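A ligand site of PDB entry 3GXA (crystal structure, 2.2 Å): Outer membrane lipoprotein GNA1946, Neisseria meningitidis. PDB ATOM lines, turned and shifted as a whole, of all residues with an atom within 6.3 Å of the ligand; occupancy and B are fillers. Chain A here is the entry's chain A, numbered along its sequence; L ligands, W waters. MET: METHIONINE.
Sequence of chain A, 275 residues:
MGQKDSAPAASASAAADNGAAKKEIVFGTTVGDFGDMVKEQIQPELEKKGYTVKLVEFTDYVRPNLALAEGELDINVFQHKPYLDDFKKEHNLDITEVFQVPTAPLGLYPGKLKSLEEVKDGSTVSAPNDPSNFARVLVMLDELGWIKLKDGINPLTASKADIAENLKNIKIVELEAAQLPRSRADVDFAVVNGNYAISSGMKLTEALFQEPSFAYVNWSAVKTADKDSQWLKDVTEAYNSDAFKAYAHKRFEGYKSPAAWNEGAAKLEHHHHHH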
ATOM      1  N   THR A  30     -27.262  -4.881 -13.570  1.00  0.00           N
ATOM      2  CA  THR A  30     -28.638  -5.355 -13.626  1.00  0.00           C
ATOM      3  C   THR A  30     -28.708  -6.324 -12.457  1.00  0.00           C
ATOM      4  O   THR A  30     -27.676  -6.824 -11.997  1.00  0.00           O
ATOM      5  CB  THR A  30     -28.974  -6.124 -14.933  1.00  0.00           C
ATOM      6  OG1 THR A  30     -27.851  -6.909 -15.357  1.00  0.00           O
ATOM      7  CG2 THR A  30     -29.395  -5.139 -16.034  1.00  0.00           C
ATOM      8  N   PHE A  34     -24.597 -10.314 -12.838  1.00  0.00           N
ATOM      9  CA  PHE A  34     -23.566  -9.282 -12.850  1.00  0.00           C
ATOM     10  C   PHE A  34     -23.387  -8.656 -11.462  1.00  0.00           C
ATOM     11  O   PHE A  34     -22.284  -8.273 -11.081  1.00  0.00           O
ATOM     12  CB  PHE A  34     -23.880  -8.217 -13.898  1.00  0.00           C
ATOM     13  CG  PHE A  34     -23.792  -8.732 -15.319  1.00  0.00           C
ATOM     14  CD1 PHE A  34     -22.747  -9.582 -15.698  1.00  0.00           C
ATOM     15  CD2 PHE A  34     -24.733  -8.364 -16.266  1.00  0.00           C
ATOM     16  CE1 PHE A  34     -22.652 -10.063 -17.003  1.00  0.00           C
ATOM     17  CE2 PHE A  34     -24.649  -8.837 -17.581  1.00  0.00           C
ATOM     18  CZ  PHE A  34     -23.604  -9.687 -17.950  1.00  0.00           C
ATOM     19  N   TYR A  61     -32.791  -1.858 -18.395  1.00  0.00           N
ATOM     20  CA  TYR A  61     -31.615  -1.593 -19.217  1.00  0.00           C
ATOM     21  C   TYR A  61     -31.388  -0.100 -19.460  1.00  0.00           C
ATOM     22  O   TYR A  61     -30.299   0.311 -19.848  1.00  0.00           O
ATOM     23  CB  TYR A  61     -31.743  -2.291 -20.580  1.00  0.00           C
ATOM     24  CG  TYR A  61     -31.687  -3.816 -20.589  1.00  0.00           C
ATOM     25  CD1 TYR A  61     -31.032  -4.537 -19.578  1.00  0.00           C
ATOM     26  CD2 TYR A  61     -32.209  -4.543 -21.664  1.00  0.00           C
ATOM     27  CE1 TYR A  61     -30.906  -5.938 -19.647  1.00  0.00           C
ATOM     28  CE2 TYR A  61     -32.085  -5.925 -21.746  1.00  0.00           C
ATOM     29  CZ  TYR A  61     -31.435  -6.618 -20.748  1.00  0.00           C
ATOM     30  OH  TYR A  61     -31.305  -7.980 -20.842  1.00  0.00           O
ATOM     31  N   PHE A  78     -23.611  -4.387 -17.577  1.00  0.00           N
ATOM     32  CA  PHE A  78     -24.933  -4.922 -17.883  1.00  0.00           C
ATOM     33  C   PHE A  78     -25.291  -4.964 -19.374  1.00  0.00           C
ATOM     34  O   PHE A  78     -26.321  -5.517 -19.732  1.00  0.00           O
ATOM     35  CB  PHE A  78     -25.986  -4.078 -17.169  1.00  0.00           C
ATOM     36  CG  PHE A  78     -26.344  -2.812 -17.904  1.00  0.00           C
ATOM     37  CD1 PHE A  78     -27.488  -2.748 -18.698  1.00  0.00           C
ATOM     38  CD2 PHE A  78     -25.489  -1.707 -17.869  1.00  0.00           C
ATOM     39  CE1 PHE A  78     -27.793  -1.599 -19.444  1.00  0.00           C
ATOM     40  CE2 PHE A  78     -25.785  -0.557 -18.616  1.00  0.00           C
ATOM     41  CZ  PHE A  78     -26.936  -0.502 -19.398  1.00  0.00           C
ATOM     42  N   GLN A  79     -24.468  -4.393 -20.234  1.00  0.00           N
ATOM     43  CA  GLN A  79     -24.809  -4.344 -21.657  1.00  0.00           C
ATOM     44  C   GLN A  79     -23.730  -4.836 -22.615  1.00  0.00           C
ATOM     45  O   GLN A  79     -22.580  -5.025 -22.232  1.00  0.00           O
ATOM     46  CB  GLN A  79     -25.125  -2.894 -22.032  1.00  0.00           C
ATOM     47  CG  GLN A  79     -23.861  -2.037 -22.153  1.00  0.00           C
ATOM     48  CD  GLN A  79     -24.096  -0.565 -21.851  1.00  0.00           C
ATOM     49  OE1 GLN A  79     -23.443   0.007 -20.971  1.00  0.00           O
ATOM     50  NE2 GLN A  79     -25.017   0.072 -22.578  1.00  0.00           N
ATOM     51  N   HIS A  80     -24.129  -5.020 -23.865  1.00  0.00           N
ATOM     52  CA  HIS A  80     -23.168  -5.423 -24.895  1.00  0.00           C
ATOM     53  C   HIS A  80     -22.823  -4.155 -25.677  1.00  0.00           C
ATOM     54  O   HIS A  80     -23.483  -3.136 -25.510  1.00  0.00           O
ATOM     55  CB  HIS A  80     -23.739  -6.533 -25.790  1.00  0.00           C
ATOM     56  CG  HIS A  80     -25.163  -6.351 -26.192  1.00  0.00           C
ATOM     57  ND1 HIS A  80     -25.573  -5.360 -27.062  1.00  0.00           N
ATOM     58  CD2 HIS A  80     -26.275  -7.069 -25.898  1.00  0.00           C
ATOM     59  CE1 HIS A  80     -26.874  -5.488 -27.286  1.00  0.00           C
ATOM     60  NE2 HIS A  80     -27.316  -6.515 -26.596  1.00  0.00           N
ATOM     61  N   TYR A  83     -25.484  -2.248 -27.836  1.00  0.00           N
ATOM     62  CA  TYR A  83     -26.473  -1.539 -27.041  1.00  0.00           C
ATOM     63  C   TYR A  83     -25.837  -0.248 -26.525  1.00  0.00           C
ATOM     64  O   TYR A  83     -26.440   0.816 -26.570  1.00  0.00           O
ATOM     65  CB  TYR A  83     -26.971  -2.390 -25.871  1.00  0.00           C
ATOM     66  CG  TYR A  83     -28.065  -1.736 -25.082  1.00  0.00           C
ATOM     67  CD1 TYR A  83     -27.779  -0.794 -24.094  1.00  0.00           C
ATOM     68  CD2 TYR A  83     -29.409  -1.988 -25.379  1.00  0.00           C
ATOM     69  CE1 TYR A  83     -28.784  -0.129 -23.413  1.00  0.00           C
ATOM     70  CE2 TYR A  83     -30.435  -1.306 -24.699  1.00  0.00           C
ATOM     71  CZ  TYR A  83     -30.108  -0.380 -23.722  1.00  0.00           C
ATOM     72  OH  TYR A  83     -31.093   0.297 -23.035  1.00  0.00           O
ATOM     73  N   LEU A  84     -24.606  -0.367 -26.055  1.00  0.00           N
ATOM     74  CA  LEU A  84     -23.885   0.792 -25.551  1.00  0.00           C
ATOM     75  C   LEU A  84     -23.838   1.847 -26.647  1.00  0.00           C
ATOM     76  O   LEU A  84     -24.186   3.012 -26.432  1.00  0.00           O
ATOM     77  CB  LEU A  84     -22.449   0.406 -25.177  1.00  0.00           C
ATOM     78  CG  LEU A  84     -21.730   1.135 -24.037  1.00  0.00           C
ATOM     79  CD1 LEU A  84     -20.235   1.045 -24.279  1.00  0.00           C
ATOM     80  CD2 LEU A  84     -22.172   2.579 -23.938  1.00  0.00           C
ATOM     81  N   THR A 103     -20.772 -13.609 -19.802  1.00  0.00           N
ATOM     82  CA  THR A 103     -22.171 -13.253 -19.933  1.00  0.00           C
ATOM     83  C   THR A 103     -23.111 -14.370 -20.353  1.00  0.00           C
ATOM     84  O   THR A 103     -22.755 -15.222 -21.171  1.00  0.00           O
ATOM     85  CB  THR A 103     -22.375 -12.000 -20.870  1.00  0.00           C
ATOM     86  OG1 THR A 103     -23.049 -12.397 -22.083  1.00  0.00           O
ATOM     87  CG2 THR A 103     -21.055 -11.372 -21.211  1.00  0.00           C
ATOM     88  N   ALA A 104     -24.300 -14.367 -19.763  1.00  0.00           N
ATOM     89  CA  ALA A 104     -25.324 -15.370 -20.069  1.00  0.00           C
ATOM     90  C   ALA A 104     -25.758 -15.164 -21.522  1.00  0.00           C
ATOM     91  O   ALA A 104     -26.164 -14.070 -21.900  1.00  0.00           O
ATOM     92  CB  ALA A 104     -26.516 -15.218 -19.122  1.00  0.00           C
ATOM     93  N   PRO A 105     -25.671 -16.213 -22.336  1.00  0.00           N
ATOM     94  CA  PRO A 105     -26.053 -16.157 -23.746  1.00  0.00           C
ATOM     95  C   PRO A 105     -27.534 -16.012 -24.048  1.00  0.00           C
ATOM     96  O   PRO A 105     -28.382 -16.443 -23.273  1.00  0.00           O
ATOM     97  CB  PRO A 105     -25.488 -17.463 -24.306  1.00  0.00           C
ATOM     98  CG  PRO A 105     -25.604 -18.398 -23.148  1.00  0.00           C
ATOM     99  CD  PRO A 105     -25.129 -17.547 -21.992  1.00  0.00           C
ATOM    100  N   LEU A 106     -27.837 -15.370 -25.179  1.00  0.00           N
ATOM    101  CA  LEU A 106     -29.213 -15.195 -25.614  1.00  0.00           C
ATOM    102  C   LEU A 106     -29.708 -16.559 -26.122  1.00  0.00           C
ATOM    103  O   LEU A 106     -29.001 -17.237 -26.858  1.00  0.00           O
ATOM    104  CB  LEU A 106     -29.277 -14.180 -26.757  1.00  0.00           C
ATOM    105  CG  LEU A 106     -30.669 -13.900 -27.334  1.00  0.00           C
ATOM    106  CD1 LEU A 106     -31.504 -13.175 -26.281  1.00  0.00           C
ATOM    107  CD2 LEU A 106     -30.563 -13.059 -28.602  1.00  0.00           C
ATOM    108  N   ASP A 130     -36.262  -3.495 -27.762  1.00  0.00           N
ATOM    109  CA  ASP A 130     -35.254  -2.474 -28.033  1.00  0.00           C
ATOM    110  C   ASP A 130     -34.494  -2.977 -29.288  1.00  0.00           C
ATOM    111  O   ASP A 130     -34.187  -4.158 -29.417  1.00  0.00           O
ATOM    112  CB  ASP A 130     -34.304  -2.299 -26.847  1.00  0.00           C
ATOM    113  CG  ASP A 130     -33.630  -3.590 -26.448  1.00  0.00           C
ATOM    114  OD1 ASP A 130     -34.313  -4.479 -25.896  1.00  0.00           O
ATOM    115  OD2 ASP A 130     -32.424  -3.727 -26.701  1.00  0.00           O
ATOM    116  N   SER A 132     -31.224  -2.912 -30.670  1.00  0.00           N
ATOM    117  CA  SER A 132     -29.997  -3.708 -30.655  1.00  0.00           C
ATOM    118  C   SER A 132     -30.236  -5.167 -30.274  1.00  0.00           C
ATOM    119  O   SER A 132     -29.586  -6.065 -30.818  1.00  0.00           O
ATOM    120  CB  SER A 132     -28.953  -3.072 -29.733  1.00  0.00           C
ATOM    121  OG  SER A 132     -29.331  -3.158 -28.369  1.00  0.00           O
ATOM    122  N   ASN A 133     -31.151  -5.419 -29.353  1.00  0.00           N
ATOM    123  CA  ASN A 133     -31.460  -6.783 -28.948  1.00  0.00           C
ATOM    124  C   ASN A 133     -32.440  -7.465 -29.900  1.00  0.00           C
ATOM    125  O   ASN A 133     -32.361  -8.675 -30.129  1.00  0.00           O
ATOM    126  CB  ASN A 133     -31.992  -6.779 -27.511  1.00  0.00           C
ATOM    127  CG  ASN A 133     -30.888  -6.662 -26.483  1.00  0.00           C
ATOM    128  OD1 ASN A 133     -30.088  -7.577 -26.319  1.00  0.00           O
ATOM    129  ND2 ASN A 133     -30.826  -5.517 -25.803  1.00  0.00           N
ATOM    130  N   ARG A 136     -30.857  -9.211 -32.864  1.00  0.00           N
ATOM    131  CA  ARG A 136     -30.338 -10.529 -32.530  1.00  0.00           C
ATOM    132  C   ARG A 136     -31.375 -11.617 -32.765  1.00  0.00           C
ATOM    133  O   ARG A 136     -31.061 -12.702 -33.239  1.00  0.00           O
ATOM    134  CB  ARG A 136     -29.899 -10.591 -31.064  1.00  0.00           C
ATOM    135  CG  ARG A 136     -28.793  -9.641 -30.698  1.00  0.00           C
ATOM    136  CD  ARG A 136     -27.931 -10.258 -29.615  1.00  0.00           C
ATOM    137  NE  ARG A 136     -28.406  -9.964 -28.278  1.00  0.00           N
ATOM    138  CZ  ARG A 136     -27.932 -10.536 -27.169  1.00  0.00           C
ATOM    139  NH1 ARG A 136     -26.972 -11.444 -27.231  1.00  0.00           N
ATOM    140  NH2 ARG A 136     -28.413 -10.149 -26.003  1.00  0.00           N
ATOM    141  N   VAL A 192     -35.197 -15.042 -24.756  1.00  0.00           N
ATOM    142  CA  VAL A 192     -34.916 -14.299 -23.532  1.00  0.00           C
ATOM    143  C   VAL A 192     -33.468 -13.868 -23.305  1.00  0.00           C
ATOM    144  O   VAL A 192     -32.551 -14.672 -23.477  1.00  0.00           O
ATOM    145  CB  VAL A 192     -35.346 -15.176 -22.315  1.00  0.00           C
ATOM    146  CG1 VAL A 192     -35.275 -14.391 -21.018  1.00  0.00           C
ATOM    147  CG2 VAL A 192     -36.747 -15.766 -22.568  1.00  0.00           C
ATOM    148  N   ASN A 193     -33.266 -12.606 -22.923  1.00  0.00           N
ATOM    149  CA  ASN A 193     -31.919 -12.130 -22.632  1.00  0.00           C
ATOM    150  C   ASN A 193     -31.457 -12.969 -21.441  1.00  0.00           C
ATOM    151  O   ASN A 193     -32.248 -13.257 -20.535  1.00  0.00           O
ATOM    152  CB  ASN A 193     -31.907 -10.640 -22.261  1.00  0.00           C
ATOM    153  CG  ASN A 193     -32.186  -9.727 -23.446  1.00  0.00           C
ATOM    154  OD1 ASN A 193     -33.330  -9.461 -23.779  1.00  0.00           O
ATOM    155  ND2 ASN A 193     -31.127  -9.277 -24.099  1.00  0.00           N
ATOM    156  N   GLY A 194     -30.188 -13.356 -21.447  1.00  0.00           N
ATOM    157  CA  GLY A 194     -29.658 -14.190 -20.393  1.00  0.00           C
ATOM    158  C   GLY A 194     -29.830 -13.736 -18.967  1.00  0.00           C
ATOM    159  O   GLY A 194     -30.212 -14.524 -18.097  1.00  0.00           O
ATOM    160  N   ASN A 195     -29.529 -12.464 -18.705  1.00  0.00           N
ATOM    161  CA  ASN A 195     -29.625 -11.938 -17.355  1.00  0.00           C
ATOM    162  C   ASN A 195     -31.033 -12.078 -16.801  1.00  0.00           C
ATOM    163  O   ASN A 195     -31.195 -12.337 -15.617  1.00  0.00           O
ATOM    164  CB  ASN A 195     -29.177 -10.468 -17.320  1.00  0.00           C
ATOM    165  CG  ASN A 195     -30.158  -9.539 -17.995  1.00  0.00           C
ATOM    166  OD1 ASN A 195     -30.159  -9.385 -19.215  1.00  0.00           O
ATOM    167  ND2 ASN A 195     -30.996  -8.902 -17.194  1.00  0.00           N
ATOM    168  N   TYR A 216     -21.902 -10.182 -28.745  1.00  0.00           N
ATOM    169  CA  TYR A 216     -22.723  -9.587 -27.698  1.00  0.00           C
ATOM    170  C   TYR A 216     -22.277  -9.916 -26.272  1.00  0.00           C
ATOM    171  O   TYR A 216     -23.071  -9.805 -25.332  1.00  0.00           O
ATOM    172  CB  TYR A 216     -24.182  -9.987 -27.908  1.00  0.00           C
ATOM    173  CG  TYR A 216     -24.763  -9.415 -29.180  1.00  0.00           C
ATOM    174  CD1 TYR A 216     -25.319  -8.141 -29.213  1.00  0.00           C
ATOM    175  CD2 TYR A 216     -24.738 -10.156 -30.368  1.00  0.00           C
ATOM    176  CE1 TYR A 216     -25.836  -7.612 -30.394  1.00  0.00           C
ATOM    177  CE2 TYR A 216     -25.254  -9.639 -31.559  1.00  0.00           C
ATOM    178  CZ  TYR A 216     -25.798  -8.360 -31.563  1.00  0.00           C
ATOM    179  OH  TYR A 216     -26.300  -7.858 -32.722  1.00  0.00           O
ATOM    180  N   VAL A 217     -21.022 -10.329 -26.123  1.00  0.00           N
ATOM    181  CA  VAL A 217     -20.481 -10.606 -24.801  1.00  0.00           C
ATOM    182  C   VAL A 217     -20.453  -9.208 -24.168  1.00  0.00           C
ATOM    183  O   VAL A 217     -19.941  -8.263 -24.754  1.00  0.00           O
ATOM    184  CB  VAL A 217     -19.065 -11.196 -24.886  1.00  0.00           C
ATOM    185  CG1 VAL A 217     -18.502 -11.422 -23.481  1.00  0.00           C
ATOM    186  CG2 VAL A 217     -19.107 -12.500 -25.660  1.00  0.00           C
ATOM    187  N   ASN A 218     -21.022  -9.093 -22.984  1.00  0.00           N
ATOM    188  CA  ASN A 218     -21.108  -7.805 -22.299  1.00  0.00           C
ATOM    189  C   ASN A 218     -19.800  -7.159 -21.884  1.00  0.00           C
ATOM    190  O   ASN A 218     -18.798  -7.826 -21.624  1.00  0.00           O
ATOM    191  CB  ASN A 218     -22.042  -7.938 -21.097  1.00  0.00           C
ATOM    192  CG  ASN A 218     -23.474  -8.214 -21.516  1.00  0.00           C
ATOM    193  OD1 ASN A 218     -24.407  -7.939 -20.766  1.00  0.00           O
ATOM    194  ND2 ASN A 218     -23.655  -8.761 -22.720  1.00  0.00           N
HETATM  195  N   MET L   1     -27.161  -9.011 -20.419  1.00  0.00           N
HETATM  196  CA  MET L   1     -27.886  -8.670 -21.683  1.00  0.00           C
HETATM  197  C   MET L   1     -27.494  -9.641 -22.803  1.00  0.00           C
HETATM  198  O   MET L   1     -26.289  -9.927 -22.928  1.00  0.00           O
HETATM  199  CB  MET L   1     -27.559  -7.235 -22.119  1.00  0.00           C
HETATM  200  CG  MET L   1     -28.490  -6.708 -23.196  1.00  0.00           C
HETATM  201  SD  MET L   1     -28.056  -5.058 -23.736  1.00  0.00           S
HETATM  202  CE  MET L   1     -28.563  -4.079 -22.315  1.00  0.00           C
HETATM  203  OXT MET L   1     -28.407 -10.107 -23.524  1.00  0.00           O
HETATM  204  O   HOH W   1     -27.881  -7.137 -18.327  1.00  0.00           O
HETATM  205  O   HOH W   2     -25.982 -12.179 -24.074  1.00  0.00           O
HETATM  206  O   HOH W   3     -28.918 -12.692 -23.778  1.00  0.00           O
HETATM  207  O   HOH W   4     -27.021 -11.919 -20.284  1.00  0.00           O
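A ring nitrogen (ND1) of His 80 is in hydrogen-bond range of the backbone NH (N) of Tyr 83, 3.2 Å away. OD1 of Asn 133 lies within hydrogen-bond range of NE2 of His 80 (3.0 Å). The backbone carbonyl oxygen of Tyr 61 lies within hydrogen-bond range of the side-chain hydroxyl of Tyr 83, at 3.3 Å. ND2 of Asn 133 lies within hydrogen-bond range of OD2 of Asp 130 (2.6 Å). The backbone carbonyl oxygen (O) of Phe 78 lies close to the side-chain amide oxygen (OD1) of Asn 218 (3.3 Å). O of Tyr 216 sits at hydrogen-bond distance from ND2 of Asn 218 (2.9 Å). The side-chain amide nitrogen of Asn 193 sits at hydrogen-bond distance from the side-chain amide oxygen of Asn 133 (3.0 Å). The side-chain hydroxyl (OH) of Tyr 61 sits at hydrogen-bond distance from the side-chain amide oxygen (OD1) of Asn 195, 2.4 Å away.
CE2 of Phe 34 touches N of the ligand (3.8 Å). Tyr 61 touches the ligand. Phe 78 touches the ligand (O to CB, 3.2 Å). Gln 79 touches the ligand. Tyr 83 touches the ligand. Hydrophobic or aromatic side chains within 4 Å of the ligand: Phe 34, Tyr 61, Phe 78, His 80 and Tyr 83. 11 residues have an atom within 4 Å of the ligand: Phe 34, Tyr 61, Phe 78, Gln 79, His 80, Tyr 83, Asn 133, Arg 136, Asn 193, Asn 195 and Asn 218. The nearest printed residue that does not touch the ligand is Tyr 216 (4.02 Å).
Water W2 lies within hydrogen-bond range of an oxygen (O) of the ligand (2.5 Å), the backbone carbonyl oxygen of Ala 104 (2.9 Å) and the guanidinium group of Arg 136 (3.4 Å). Water W1 lies within hydrogen-bond range of the backbone carbonyl oxygen of Phe 78 (2.7 Å), a nitrogen (N) of the ligand (2.9 Å), the side-chain hydroxyl of Thr 30 (3.0 Å) and the side-chain amide oxygen of Asn 195 (3.3 Å). Water W4 lies within hydrogen-bond range of O of Ala 104, N of the ligand and N of Asn 195.
NE2 of His 80 lies close to SD of the ligand. OD1 of Asn 195 is in hydrogen-bond range of N of the ligand, 3.3 Å away. ND2 of Asn 218 is in hydrogen-bond range of O of the ligand, 2.9 Å away. An oxygen (OXT) of the ligand is in hydrogen-bond range of the side-chain amide nitrogen (ND2) of Asn 193 (2.9 Å). A sulfur (SD) of the ligand lies close to the side-chain amide nitrogen (ND2) of Asn 133, 3.5 Å away. NH2 of Arg 136 lies within salt-bridge range of OXT of the ligand (2.5 Å).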
